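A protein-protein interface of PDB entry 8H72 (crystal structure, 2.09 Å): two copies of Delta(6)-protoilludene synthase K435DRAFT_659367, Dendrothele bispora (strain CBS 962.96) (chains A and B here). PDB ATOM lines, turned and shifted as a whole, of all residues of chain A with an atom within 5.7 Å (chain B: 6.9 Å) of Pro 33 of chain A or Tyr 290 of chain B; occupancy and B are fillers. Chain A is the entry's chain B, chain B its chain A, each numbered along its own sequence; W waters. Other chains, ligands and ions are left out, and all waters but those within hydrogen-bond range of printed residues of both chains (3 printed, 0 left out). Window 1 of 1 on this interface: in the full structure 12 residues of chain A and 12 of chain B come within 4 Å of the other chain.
The indole nitrogen (NE1) of Trp 34 of chain B is in hydrogen-bond range of the side-chain carboxylate (OE1) of Glu 309 of chain B, at 3.0 Å.
The backbone carbonyl oxygen of Trp 34 of chain A lies within hydrogen-bond range of the guanidinium group of Arg 316 of chain A (2.7 Å).
Of chain B, only Leu 287 (3.2 Å), Tyr 290 (3.9 Å) and Lys 291 (3.3 Å) come within 4 Å of Pro 33 of chain A.
Tyr 290 of chain B touches just these residues of chain A: Pro 33 (3.9 Å), Tyr 290 (2.6 Å) and Lys 291 (3.3 Å).
Printed residues of chain A within 4 Å of Pro 33 of chain B: Leu 287 (3.3 Å), Tyr 290 (3.8 Å) and Lys 291 (3.8 Å).
Printed residues of chain B within 4 Å of Asn 31 of chain A: Arg 288 (2.8 Å).
Printed residues of chain A within 4 Å of Lys 291 of chain B: Pro 33 (3.3 Å), Trp 34 (3.9 Å) and Pro 35 (3.7 Å).
Of the printed residues of chain A, Trp 34 of chain B touches Lys 291 (3.6 Å).
Phe 286 of chain B touches none of the printed residues of chain A.
Trp 229 of chain B touches none of the printed residues of chain A.
The nearest printed residue of chain A that does not touch Tyr 290 of chain B is Trp 34 of chain A (5.8 Å).
Water W1 lies within hydrogen-bond range of O of Pro 33 of chain A, N of Lys 291 of chain B, O of Arg 288 of chain B and N of Tyr 290 of chain B.
Water W3 lies within hydrogen-bond range of O of Leu 287 of chain A (2.8 Å), N of Lys 291 of chain A (2.8 Å), O of Pro 33 of chain B (2.9 Å) and N of Tyr 290 of chain A (3.1 Å).
Water W2 lies within hydrogen-bond range of the backbone carbonyl oxygen of Trp 32 of chain A and the backbone carbonyl oxygen of Arg 288 of chain B.
Pro 33 of chain A touches Leu 287 of chain B.
CB of Pro 33 of chain A touches CE1 of Tyr 290 of chain B, 3.9 Å away.
Pro 33 of chain A touches Lys 291 of chain B.
Lys 291 of chain B touches Trp 34 of chain A.
Pro 35 of chain A touches Lys 291 of chain B.
CA of Pro 33 of chain B touches O of Leu 287 of chain A, 3.3 Å away.
CE1 of Tyr 290 of chain A touches CB of Pro 33 of chain B (3.8 Å).
Lys 291 of chain A touches Pro 33 of chain B (CB to O, 3.8 Å).
CZ2 of Trp 34 of chain B touches CE of Lys 291 of chain A, 3.6 Å away.
Lys 291 of chain A touches Tyr 290 of chain B.
Pro 33 of chain A touches Lys 291 of chain B, and with the chains exchanged Lys 291 of chain A touches Pro 33 of chain B.
Trp 34 of chain A touches Lys 291 of chain B, and with the chains exchanged Lys 291 of chain A touches Trp 34 of chain B.
Tyr 290 of chain B touches its own counterpart, Tyr 290 of chain A.
Lys 291 of chain A touches Tyr 290 of chain B, but with the chains exchanged Tyr 290 of chain A does not touch Lys 291 of chain B (4.4 Å).
Of the 14 pairs that touch across the chains among the printed residues, 9 have their exchanged pair printed and touching as well.
The side-chain amide oxygen of Asn 31 of chain A sits at hydrogen-bond distance from the guanidinium group of Arg 288 of chain B, 2.8 Å away.
The side-chain hydroxyl (OH) of Tyr 290 of chain B is in hydrogen-bond range of the side-chain hydroxyl (OH) of Tyr 290 of chain A, 2.6 Å away.
OE1 of Glu 309 of chain B is in salt-bridge range of NZ of Lys 291 of chain A, 2.5 Å away.
Hydrophobic or aromatic side chains of chain B within 4 Å of the printed part of chain A: Pro 33, Trp 34 and Tyr 290.
Printed residues of chain A that touch a printed residue of chain B: Asn 31, Pro 33, Trp 34, Pro 35, Leu 287, Tyr 290 and Lys 291.
Hydrophobic or aromatic side chains of chain A within 4 Å of the printed part of chain B: Pro 33, Trp 34, Pro 35 and Tyr 290.
Among the printed residues, 14 pairs touch across the chains.
Among the printed residues, Asp or Glu carboxylates within 4 Å of a Lys or Arg side-chain nitrogen of the other chain: Lys 291 of chain A with Glu 309 of chain B.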
ATOM      1  N   ASN A  31       3.422  10.403 -19.920  1.00  0.00           N
ATOM      2  CA  ASN A  31       2.821   9.074 -19.815  1.00  0.00           C
ATOM      3  C   ASN A  31       3.063   8.165 -21.021  1.00  0.00           C
ATOM      4  O   ASN A  31       2.347   7.182 -21.212  1.00  0.00           O
ATOM      5  CB  ASN A  31       1.318   9.193 -19.549  1.00  0.00           C
ATOM      6  CG  ASN A  31       0.989  10.260 -18.524  1.00  0.00           C
ATOM      7  OD1 ASN A  31       1.494  10.235 -17.401  1.00  0.00           O
ATOM      8  ND2 ASN A  31       0.139  11.206 -18.905  1.00  0.00           N
ATOM      9  N   TRP A  32       4.065   8.488 -21.831  1.00  0.00           N
ATOM     10  CA  TRP A  32       4.382   7.676 -22.998  1.00  0.00           C
ATOM     11  C   TRP A  32       4.829   6.275 -22.574  1.00  0.00           C
ATOM     12  O   TRP A  32       5.710   6.145 -21.713  1.00  0.00           O
ATOM     13  CB  TRP A  32       5.484   8.381 -23.800  1.00  0.00           C
ATOM     14  CG  TRP A  32       5.865   7.764 -25.126  1.00  0.00           C
ATOM     15  CD1 TRP A  32       7.072   7.193 -25.448  1.00  0.00           C
ATOM     16  CD2 TRP A  32       5.068   7.712 -26.318  1.00  0.00           C
ATOM     17  NE1 TRP A  32       7.060   6.760 -26.758  1.00  0.00           N
ATOM     18  CE2 TRP A  32       5.846   7.073 -27.315  1.00  0.00           C
ATOM     19  CE3 TRP A  32       3.770   8.131 -26.638  1.00  0.00           C
ATOM     20  CZ2 TRP A  32       5.366   6.844 -28.607  1.00  0.00           C
ATOM     21  CZ3 TRP A  32       3.291   7.898 -27.924  1.00  0.00           C
ATOM     22  CH2 TRP A  32       4.089   7.257 -28.891  1.00  0.00           C
ATOM     23  N   PRO A  33       4.281   5.213 -23.182  1.00  0.00           N
ATOM     24  CA  PRO A  33       4.493   3.864 -22.632  1.00  0.00           C
ATOM     25  C   PRO A  33       5.915   3.350 -22.730  1.00  0.00           C
ATOM     26  O   PRO A  33       6.217   2.353 -22.068  1.00  0.00           O
ATOM     27  CB  PRO A  33       3.544   2.985 -23.461  1.00  0.00           C
ATOM     28  CG  PRO A  33       2.583   3.915 -24.093  1.00  0.00           C
ATOM     29  CD  PRO A  33       3.313   5.216 -24.286  1.00  0.00           C
ATOM     30  N   TRP A  34       6.802   3.958 -23.524  1.00  0.00           N
ATOM     31  CA  TRP A  34       8.163   3.436 -23.605  1.00  0.00           C
ATOM     32  C   TRP A  34       9.056   4.182 -22.625  1.00  0.00           C
ATOM     33  O   TRP A  34       9.190   5.407 -22.738  1.00  0.00           O
ATOM     34  CB  TRP A  34       8.721   3.539 -25.018  1.00  0.00           C
ATOM     35  CG  TRP A  34       8.139   2.496 -25.914  1.00  0.00           C
ATOM     36  CD1 TRP A  34       8.669   1.279 -26.215  1.00  0.00           C
ATOM     37  CD2 TRP A  34       6.884   2.566 -26.598  1.00  0.00           C
ATOM     38  NE1 TRP A  34       7.832   0.598 -27.059  1.00  0.00           N
ATOM     39  CE2 TRP A  34       6.726   1.364 -27.301  1.00  0.00           C
ATOM     40  CE3 TRP A  34       5.884   3.537 -26.689  1.00  0.00           C
ATOM     41  CZ2 TRP A  34       5.613   1.103 -28.091  1.00  0.00           C
ATOM     42  CZ3 TRP A  34       4.773   3.272 -27.471  1.00  0.00           C
ATOM     43  CH2 TRP A  34       4.648   2.065 -28.158  1.00  0.00           C
ATOM     44  N   PRO A  35       9.666   3.498 -21.664  1.00  0.00           N
ATOM     45  CA  PRO A  35      10.549   4.177 -20.712  1.00  0.00           C
ATOM     46  C   PRO A  35      11.944   4.386 -21.284  1.00  0.00           C
ATOM     47  O   PRO A  35      12.361   3.726 -22.242  1.00  0.00           O
ATOM     48  CB  PRO A  35      10.588   3.197 -19.536  1.00  0.00           C
ATOM     49  CG  PRO A  35      10.483   1.857 -20.201  1.00  0.00           C
ATOM     50  CD  PRO A  35       9.586   2.046 -21.404  1.00  0.00           C
ATOM     51  N   LEU A 287      -1.335   5.706 -29.837  1.00  0.00           N
ATOM     52  CA  LEU A 287      -1.844   4.804 -28.807  1.00  0.00           C
ATOM     53  C   LEU A 287      -3.101   4.087 -29.279  1.00  0.00           C
ATOM     54  O   LEU A 287      -3.277   2.890 -29.022  1.00  0.00           O
ATOM     55  CB  LEU A 287      -2.122   5.593 -27.525  1.00  0.00           C
ATOM     56  CG  LEU A 287      -0.884   6.209 -26.864  1.00  0.00           C
ATOM     57  CD1 LEU A 287      -1.261   7.008 -25.616  1.00  0.00           C
ATOM     58  CD2 LEU A 287       0.096   5.117 -26.534  1.00  0.00           C
ATOM     59  N   TYR A 290      -1.425   1.384 -32.312  1.00  0.00           N
ATOM     60  CA  TYR A 290      -0.226   0.566 -32.467  1.00  0.00           C
ATOM     61  C   TYR A 290      -0.416  -0.900 -32.079  1.00  0.00           C
ATOM     62  O   TYR A 290       0.446  -1.716 -32.412  1.00  0.00           O
ATOM     63  CB  TYR A 290       0.936   1.151 -31.678  1.00  0.00           C
ATOM     64  CG  TYR A 290       0.877   0.969 -30.175  1.00  0.00           C
ATOM     65  CD1 TYR A 290       0.102   1.819 -29.399  1.00  0.00           C
ATOM     66  CD2 TYR A 290       1.637  -0.008 -29.534  1.00  0.00           C
ATOM     67  CE1 TYR A 290       0.057   1.697 -28.026  1.00  0.00           C
ATOM     68  CE2 TYR A 290       1.605  -0.140 -28.140  1.00  0.00           C
ATOM     69  CZ  TYR A 290       0.803   0.719 -27.396  1.00  0.00           C
ATOM     70  OH  TYR A 290       0.734   0.642 -26.019  1.00  0.00           O
ATOM     71  N   LYS A 291      -1.500  -1.262 -31.398  1.00  0.00           N
ATOM     72  CA  LYS A 291      -1.767  -2.669 -31.136  1.00  0.00           C
ATOM     73  C   LYS A 291      -2.799  -3.255 -32.087  1.00  0.00           C
ATOM     74  O   LYS A 291      -3.199  -4.412 -31.915  1.00  0.00           O
ATOM     75  CB  LYS A 291      -2.217  -2.874 -29.686  1.00  0.00           C
ATOM     76  CG  LYS A 291      -1.100  -2.705 -28.672  1.00  0.00           C
ATOM     77  CD  LYS A 291      -1.642  -2.755 -27.248  1.00  0.00           C
ATOM     78  CE  LYS A 291      -0.556  -3.157 -26.250  1.00  0.00           C
ATOM     79  NZ  LYS A 291      -0.277  -4.627 -26.302  1.00  0.00           N
ATOM     80  N   ARG A 316      10.877   8.251 -27.210  1.00  0.00           N
ATOM     81  CA  ARG A 316      11.427   8.430 -25.864  1.00  0.00           C
ATOM     82  C   ARG A 316      12.903   8.802 -25.915  1.00  0.00           C
ATOM     83  O   ARG A 316      13.355   9.700 -25.196  1.00  0.00           O
ATOM     84  CB  ARG A 316      11.248   7.155 -25.046  1.00  0.00           C
ATOM     85  CG  ARG A 316      12.129   7.101 -23.802  1.00  0.00           C
ATOM     86  CD  ARG A 316      11.657   8.144 -22.781  1.00  0.00           C
ATOM     87  NE  ARG A 316      10.336   7.797 -22.266  1.00  0.00           N
ATOM     88  CZ  ARG A 316       9.480   8.652 -21.727  1.00  0.00           C
ATOM     89  NH1 ARG A 316       9.774   9.940 -21.597  1.00  0.00           N
ATOM     90  NH2 ARG A 316       8.303   8.203 -21.298  1.00  0.00           N
ATOM     91  N   PRO B  33      -5.295   1.571 -25.777  1.00  0.00           N
ATOM     92  CA  PRO B  33      -4.653   0.844 -26.878  1.00  0.00           C
ATOM     93  C   PRO B  33      -5.273  -0.512 -27.188  1.00  0.00           C
ATOM     94  O   PRO B  33      -5.252  -0.919 -28.357  1.00  0.00           O
ATOM     95  CB  PRO B  33      -3.202   0.695 -26.396  1.00  0.00           C
ATOM     96  CG  PRO B  33      -3.031   1.748 -25.345  1.00  0.00           C
ATOM     97  CD  PRO B  33      -4.355   1.857 -24.678  1.00  0.00           C
ATOM     98  N   TRP B  34      -5.813  -1.224 -26.193  1.00  0.00           N
ATOM     99  CA  TRP B  34      -6.326  -2.571 -26.425  1.00  0.00           C
ATOM    100  C   TRP B  34      -7.695  -2.499 -27.082  1.00  0.00           C
ATOM    101  O   TRP B  34      -8.627  -1.938 -26.490  1.00  0.00           O
ATOM    102  CB  TRP B  34      -6.423  -3.384 -25.127  1.00  0.00           C
ATOM    103  CG  TRP B  34      -5.102  -3.870 -24.663  1.00  0.00           C
ATOM    104  CD1 TRP B  34      -4.525  -5.072 -24.933  1.00  0.00           C
ATOM    105  CD2 TRP B  34      -4.168  -3.143 -23.854  1.00  0.00           C
ATOM    106  NE1 TRP B  34      -3.284  -5.146 -24.339  1.00  0.00           N
ATOM    107  CE2 TRP B  34      -3.042  -3.969 -23.674  1.00  0.00           C
ATOM    108  CE3 TRP B  34      -4.171  -1.864 -23.279  1.00  0.00           C
ATOM    109  CZ2 TRP B  34      -1.928  -3.565 -22.927  1.00  0.00           C
ATOM    110  CZ3 TRP B  34      -3.059  -1.460 -22.539  1.00  0.00           C
ATOM    111  CH2 TRP B  34      -1.956  -2.310 -22.372  1.00  0.00           C
ATOM    112  N   LEU B 222       5.767  -3.184  -8.950  1.00  0.00           N
ATOM    113  CA  LEU B 222       5.173  -2.619 -10.158  1.00  0.00           C
ATOM    114  C   LEU B 222       4.010  -3.478 -10.664  1.00  0.00           C
ATOM    115  O   LEU B 222       2.960  -2.944 -11.039  1.00  0.00           O
ATOM    116  CB  LEU B 222       6.227  -2.450 -11.249  1.00  0.00           C
ATOM    117  CG  LEU B 222       5.665  -1.846 -12.539  1.00  0.00           C
ATOM    118  CD1 LEU B 222       4.904  -0.556 -12.263  1.00  0.00           C
ATOM    119  CD2 LEU B 222       6.771  -1.623 -13.569  1.00  0.00           C
ATOM    120  N   LEU B 226       0.249  -2.254 -11.221  1.00  0.00           N
ATOM    121  CA  LEU B 226      -0.495  -2.388 -12.474  1.00  0.00           C
ATOM    122  C   LEU B 226      -1.834  -3.074 -12.243  1.00  0.00           C
ATOM    123  O   LEU B 226      -2.865  -2.625 -12.760  1.00  0.00           O
ATOM    124  CB  LEU B 226       0.325  -3.170 -13.498  1.00  0.00           C
ATOM    125  CG  LEU B 226       1.554  -2.445 -14.054  1.00  0.00           C
ATOM    126  CD1 LEU B 226       2.486  -3.421 -14.724  1.00  0.00           C
ATOM    127  CD2 LEU B 226       1.173  -1.309 -15.018  1.00  0.00           C
ATOM    128  N   TRP B 229      -4.152  -0.437 -10.489  1.00  0.00           N
ATOM    129  CA  TRP B 229      -4.689   0.585 -11.383  1.00  0.00           C
ATOM    130  C   TRP B 229      -5.729  -0.016 -12.324  1.00  0.00           C
ATOM    131  O   TRP B 229      -6.795   0.574 -12.542  1.00  0.00           O
ATOM    132  CB  TRP B 229      -3.550   1.259 -12.165  1.00  0.00           C
ATOM    133  CG  TRP B 229      -2.504   1.949 -11.284  1.00  0.00           C
ATOM    134  CD1 TRP B 229      -2.727   2.620 -10.112  1.00  0.00           C
ATOM    135  CD2 TRP B 229      -1.088   2.026 -11.521  1.00  0.00           C
ATOM    136  NE1 TRP B 229      -1.537   3.102  -9.605  1.00  0.00           N
ATOM    137  CE2 TRP B 229      -0.519   2.745 -10.450  1.00  0.00           C
ATOM    138  CE3 TRP B 229      -0.248   1.546 -12.531  1.00  0.00           C
ATOM    139  CZ2 TRP B 229       0.847   3.002 -10.365  1.00  0.00           C
ATOM    140  CZ3 TRP B 229       1.112   1.807 -12.445  1.00  0.00           C
ATOM    141  CH2 TRP B 229       1.642   2.529 -11.368  1.00  0.00           C
ATOM    142  N   LYS B 285      -1.009   6.276 -15.428  1.00  0.00           N
ATOM    143  CA  LYS B 285      -0.071   5.491 -14.633  1.00  0.00           C
ATOM    144  C   LYS B 285       0.096   4.090 -15.201  1.00  0.00           C
ATOM    145  O   LYS B 285       1.204   3.534 -15.196  1.00  0.00           O
ATOM    146  CB  LYS B 285      -0.548   5.414 -13.181  1.00  0.00           C
ATOM    147  CG  LYS B 285      -0.629   6.768 -12.486  1.00  0.00           C
ATOM    148  CD  LYS B 285      -0.238   6.658 -11.027  1.00  0.00           C
ATOM    149  CE  LYS B 285      -1.394   7.012 -10.125  1.00  0.00           C
ATOM    150  NZ  LYS B 285      -1.606   8.498 -10.130  1.00  0.00           N
ATOM    151  N   PHE B 286      -0.998   3.482 -15.671  1.00  0.00           N
ATOM    152  CA  PHE B 286      -0.893   2.141 -16.242  1.00  0.00           C
ATOM    153  C   PHE B 286      -0.087   2.167 -17.539  1.00  0.00           C
ATOM    154  O   PHE B 286       0.845   1.380 -17.721  1.00  0.00           O
ATOM    155  CB  PHE B 286      -2.283   1.557 -16.468  1.00  0.00           C
ATOM    156  CG  PHE B 286      -2.277   0.100 -16.873  1.00  0.00           C
ATOM    157  CD1 PHE B 286      -2.106  -0.264 -18.201  1.00  0.00           C
ATOM    158  CD2 PHE B 286      -2.437  -0.904 -15.922  1.00  0.00           C
ATOM    159  CE1 PHE B 286      -2.094  -1.613 -18.586  1.00  0.00           C
ATOM    160  CE2 PHE B 286      -2.421  -2.253 -16.297  1.00  0.00           C
ATOM    161  CZ  PHE B 286      -2.255  -2.609 -17.632  1.00  0.00           C
ATOM    162  N   LEU B 287      -0.413   3.097 -18.439  1.00  0.00           N
ATOM    163  CA  LEU B 287       0.298   3.177 -19.716  1.00  0.00           C
ATOM    164  C   LEU B 287       1.765   3.547 -19.512  1.00  0.00           C
ATOM    165  O   LEU B 287       2.652   2.977 -20.162  1.00  0.00           O
ATOM    166  CB  LEU B 287      -0.403   4.185 -20.628  1.00  0.00           C
ATOM    167  CG  LEU B 287      -1.803   3.712 -21.037  1.00  0.00           C
ATOM    168  CD1 LEU B 287      -2.534   4.714 -21.885  1.00  0.00           C
ATOM    169  CD2 LEU B 287      -1.735   2.364 -21.748  1.00  0.00           C
ATOM    170  N   ARG B 288       2.034   4.438 -18.595  1.00  0.00           N
ATOM    171  CA  ARG B 288       3.376   4.862 -18.323  1.00  0.00           C
ATOM    172  C   ARG B 288       4.262   3.729 -17.835  1.00  0.00           C
ATOM    173  O   ARG B 288       5.434   3.724 -18.096  1.00  0.00           O
ATOM    174  CB  ARG B 288       3.366   5.982 -17.299  1.00  0.00           C
ATOM    175  CG  ARG B 288       4.692   6.648 -17.024  1.00  0.00           C
ATOM    176  CD  ARG B 288       4.602   7.560 -15.812  1.00  0.00           C
ATOM    177  NE  ARG B 288       3.385   8.349 -15.794  1.00  0.00           N
ATOM    178  CZ  ARG B 288       2.624   8.532 -14.729  1.00  0.00           C
ATOM    179  NH1 ARG B 288       2.949   7.982 -13.585  1.00  0.00           N
ATOM    180  NH2 ARG B 288       1.542   9.261 -14.807  1.00  0.00           N
ATOM    181  N   ASN B 289       3.682   2.749 -17.177  1.00  0.00           N
ATOM    182  CA  ASN B 289       4.452   1.681 -16.595  1.00  0.00           C
ATOM    183  C   ASN B 289       4.349   0.263 -17.119  1.00  0.00           C
ATOM    184  O   ASN B 289       5.151  -0.538 -16.770  1.00  0.00           O
ATOM    185  CB  ASN B 289       4.157   1.643 -15.096  1.00  0.00           C
ATOM    186  CG  ASN B 289       4.727   2.827 -14.352  1.00  0.00           C
ATOM    187  OD1 ASN B 289       5.892   2.898 -14.124  1.00  0.00           O
ATOM    188  ND2 ASN B 289       3.890   3.734 -13.975  1.00  0.00           N
ATOM    189  N   TYR B 290       3.388  -0.043 -17.960  1.00  0.00           N
ATOM    190  CA  TYR B 290       3.219  -1.407 -18.396  1.00  0.00           C
ATOM    191  C   TYR B 290       4.352  -2.073 -19.141  1.00  0.00           C
ATOM    192  O   TYR B 290       4.377  -3.227 -19.191  1.00  0.00           O
ATOM    193  CB  TYR B 290       1.884  -1.660 -19.039  1.00  0.00           C
ATOM    194  CG  TYR B 290       1.850  -1.584 -20.524  1.00  0.00           C
ATOM    195  CD1 TYR B 290       1.736  -0.381 -21.166  1.00  0.00           C
ATOM    196  CD2 TYR B 290       1.866  -2.719 -21.288  1.00  0.00           C
ATOM    197  CE1 TYR B 290       1.675  -0.310 -22.529  1.00  0.00           C
ATOM    198  CE2 TYR B 290       1.792  -2.653 -22.647  1.00  0.00           C
ATOM    199  CZ  TYR B 290       1.707  -1.452 -23.263  1.00  0.00           C
ATOM    200  OH  TYR B 290       1.650  -1.399 -24.606  1.00  0.00           O
ATOM    201  N   LYS B 291       5.299  -1.313 -19.656  1.00  0.00           N
ATOM    202  CA  LYS B 291       6.460  -1.859 -20.337  1.00  0.00           C
ATOM    203  C   LYS B 291       7.703  -1.514 -19.522  1.00  0.00           C
ATOM    204  O   LYS B 291       8.809  -1.460 -20.059  1.00  0.00           O
ATOM    205  CB  LYS B 291       6.574  -1.287 -21.751  1.00  0.00           C
ATOM    206  CG  LYS B 291       5.257  -1.239 -22.509  1.00  0.00           C
ATOM    207  CD  LYS B 291       5.362  -0.357 -23.743  1.00  0.00           C
ATOM    208  CE  LYS B 291       4.644  -0.979 -24.929  1.00  0.00           C
ATOM    209  NZ  LYS B 291       5.384  -2.151 -25.473  1.00  0.00           N
ATOM    210  N   ASN B 292       7.516  -1.282 -18.224  1.00  0.00           N
ATOM    211  CA  ASN B 292       8.638  -0.927 -17.348  1.00  0.00           C
ATOM    212  C   ASN B 292       9.090  -1.991 -16.337  1.00  0.00           C
ATOM    213  O   ASN B 292       9.886  -1.698 -15.445  1.00  0.00           O
ATOM    214  CB  ASN B 292       8.337   0.383 -16.612  1.00  0.00           C
ATOM    215  CG  ASN B 292       9.584   1.204 -16.350  1.00  0.00           C
ATOM    216  OD1 ASN B 292      10.619   1.003 -16.986  1.00  0.00           O
ATOM    217  ND2 ASN B 292       9.492   2.136 -15.409  1.00  0.00           N
ATOM    218  N   MET B 293       8.590  -3.215 -16.471  1.00  0.00           N
ATOM    219  CA  MET B 293       8.971  -4.296 -15.565  1.00  0.00           C
ATOM    220  C   MET B 293      10.446  -4.659 -15.743  1.00  0.00           C
ATOM    221  O   MET B 293      10.967  -4.626 -16.863  1.00  0.00           O
ATOM    222  CB  MET B 293       8.112  -5.545 -15.805  1.00  0.00           C
ATOM    223  CG  MET B 293       6.698  -5.517 -15.221  1.00  0.00           C
ATOM    224  SD  MET B 293       6.592  -5.535 -13.404  1.00  0.00           S
ATOM    225  CE  MET B 293       7.048  -7.213 -12.982  1.00  0.00           C
ATOM    226  N   VAL B 304       5.236 -12.526 -17.738  1.00  0.00           N
ATOM    227  CA  VAL B 304       4.904 -11.197 -17.228  1.00  0.00           C
ATOM    228  C   VAL B 304       4.266 -10.348 -18.321  1.00  0.00           C
ATOM    229  O   VAL B 304       3.261  -9.661 -18.091  1.00  0.00           O
ATOM    230  CB  VAL B 304       6.173 -10.527 -16.658  1.00  0.00           C
ATOM    231  CG1 VAL B 304       5.953  -9.022 -16.381  1.00  0.00           C
ATOM    232  CG2 VAL B 304       6.628 -11.255 -15.391  1.00  0.00           C
ATOM    233  N   THR B 305       4.843 -10.372 -19.526  1.00  0.00           N
ATOM    234  CA  THR B 305       4.288  -9.575 -20.616  1.00  0.00           C
ATOM    235  C   THR B 305       2.873 -10.025 -20.956  1.00  0.00           C
ATOM    236  O   THR B 305       1.959  -9.200 -21.083  1.00  0.00           O
ATOM    237  CB  THR B 305       5.184  -9.663 -21.851  1.00  0.00           C
ATOM    238  OG1 THR B 305       6.491  -9.177 -21.523  1.00  0.00           O
ATOM    239  CG2 THR B 305       4.590  -8.815 -22.977  1.00  0.00           C
ATOM    240  N   ILE B 308       0.391  -8.955 -18.222  1.00  0.00           N
ATOM    241  CA  ILE B 308       0.026  -7.545 -18.312  1.00  0.00           C
ATOM    242  C   ILE B 308      -0.869  -7.299 -19.523  1.00  0.00           C
ATOM    243  O   ILE B 308      -1.799  -6.486 -19.463  1.00  0.00           O
ATOM    244  CB  ILE B 308       1.292  -6.665 -18.343  1.00  0.00           C
ATOM    245  CG1 ILE B 308       2.066  -6.798 -17.020  1.00  0.00           C
ATOM    246  CG2 ILE B 308       0.947  -5.186 -18.610  1.00  0.00           C
ATOM    247  CD1 ILE B 308       3.476  -6.261 -17.086  1.00  0.00           C
ATOM    248  N   GLU B 309      -0.613  -7.996 -20.634  1.00  0.00           N
ATOM    249  CA  GLU B 309      -1.525  -7.898 -21.771  1.00  0.00           C
ATOM    250  C   GLU B 309      -2.951  -8.272 -21.364  1.00  0.00           C
ATOM    251  O   GLU B 309      -3.922  -7.650 -21.817  1.00  0.00           O
ATOM    252  CB  GLU B 309      -1.049  -8.792 -22.920  1.00  0.00           C
ATOM    253  CG  GLU B 309       0.187  -8.297 -23.680  1.00  0.00           C
ATOM    254  CD  GLU B 309       0.004  -6.912 -24.279  1.00  0.00           C
ATOM    255  OE1 GLU B 309      -0.896  -6.751 -25.116  1.00  0.00           O
ATOM    256  OE2 GLU B 309       0.738  -5.974 -23.895  1.00  0.00           O
HETATM  257  O   HOH W   1       5.704   1.304 -19.745  1.00  0.00           O
HETATM  258  O   HOH W   2       7.403   4.991 -19.738  1.00  0.00           O
HETATM  259  O   HOH W   3      -3.506   0.377 -30.250  1.00  0.00           O
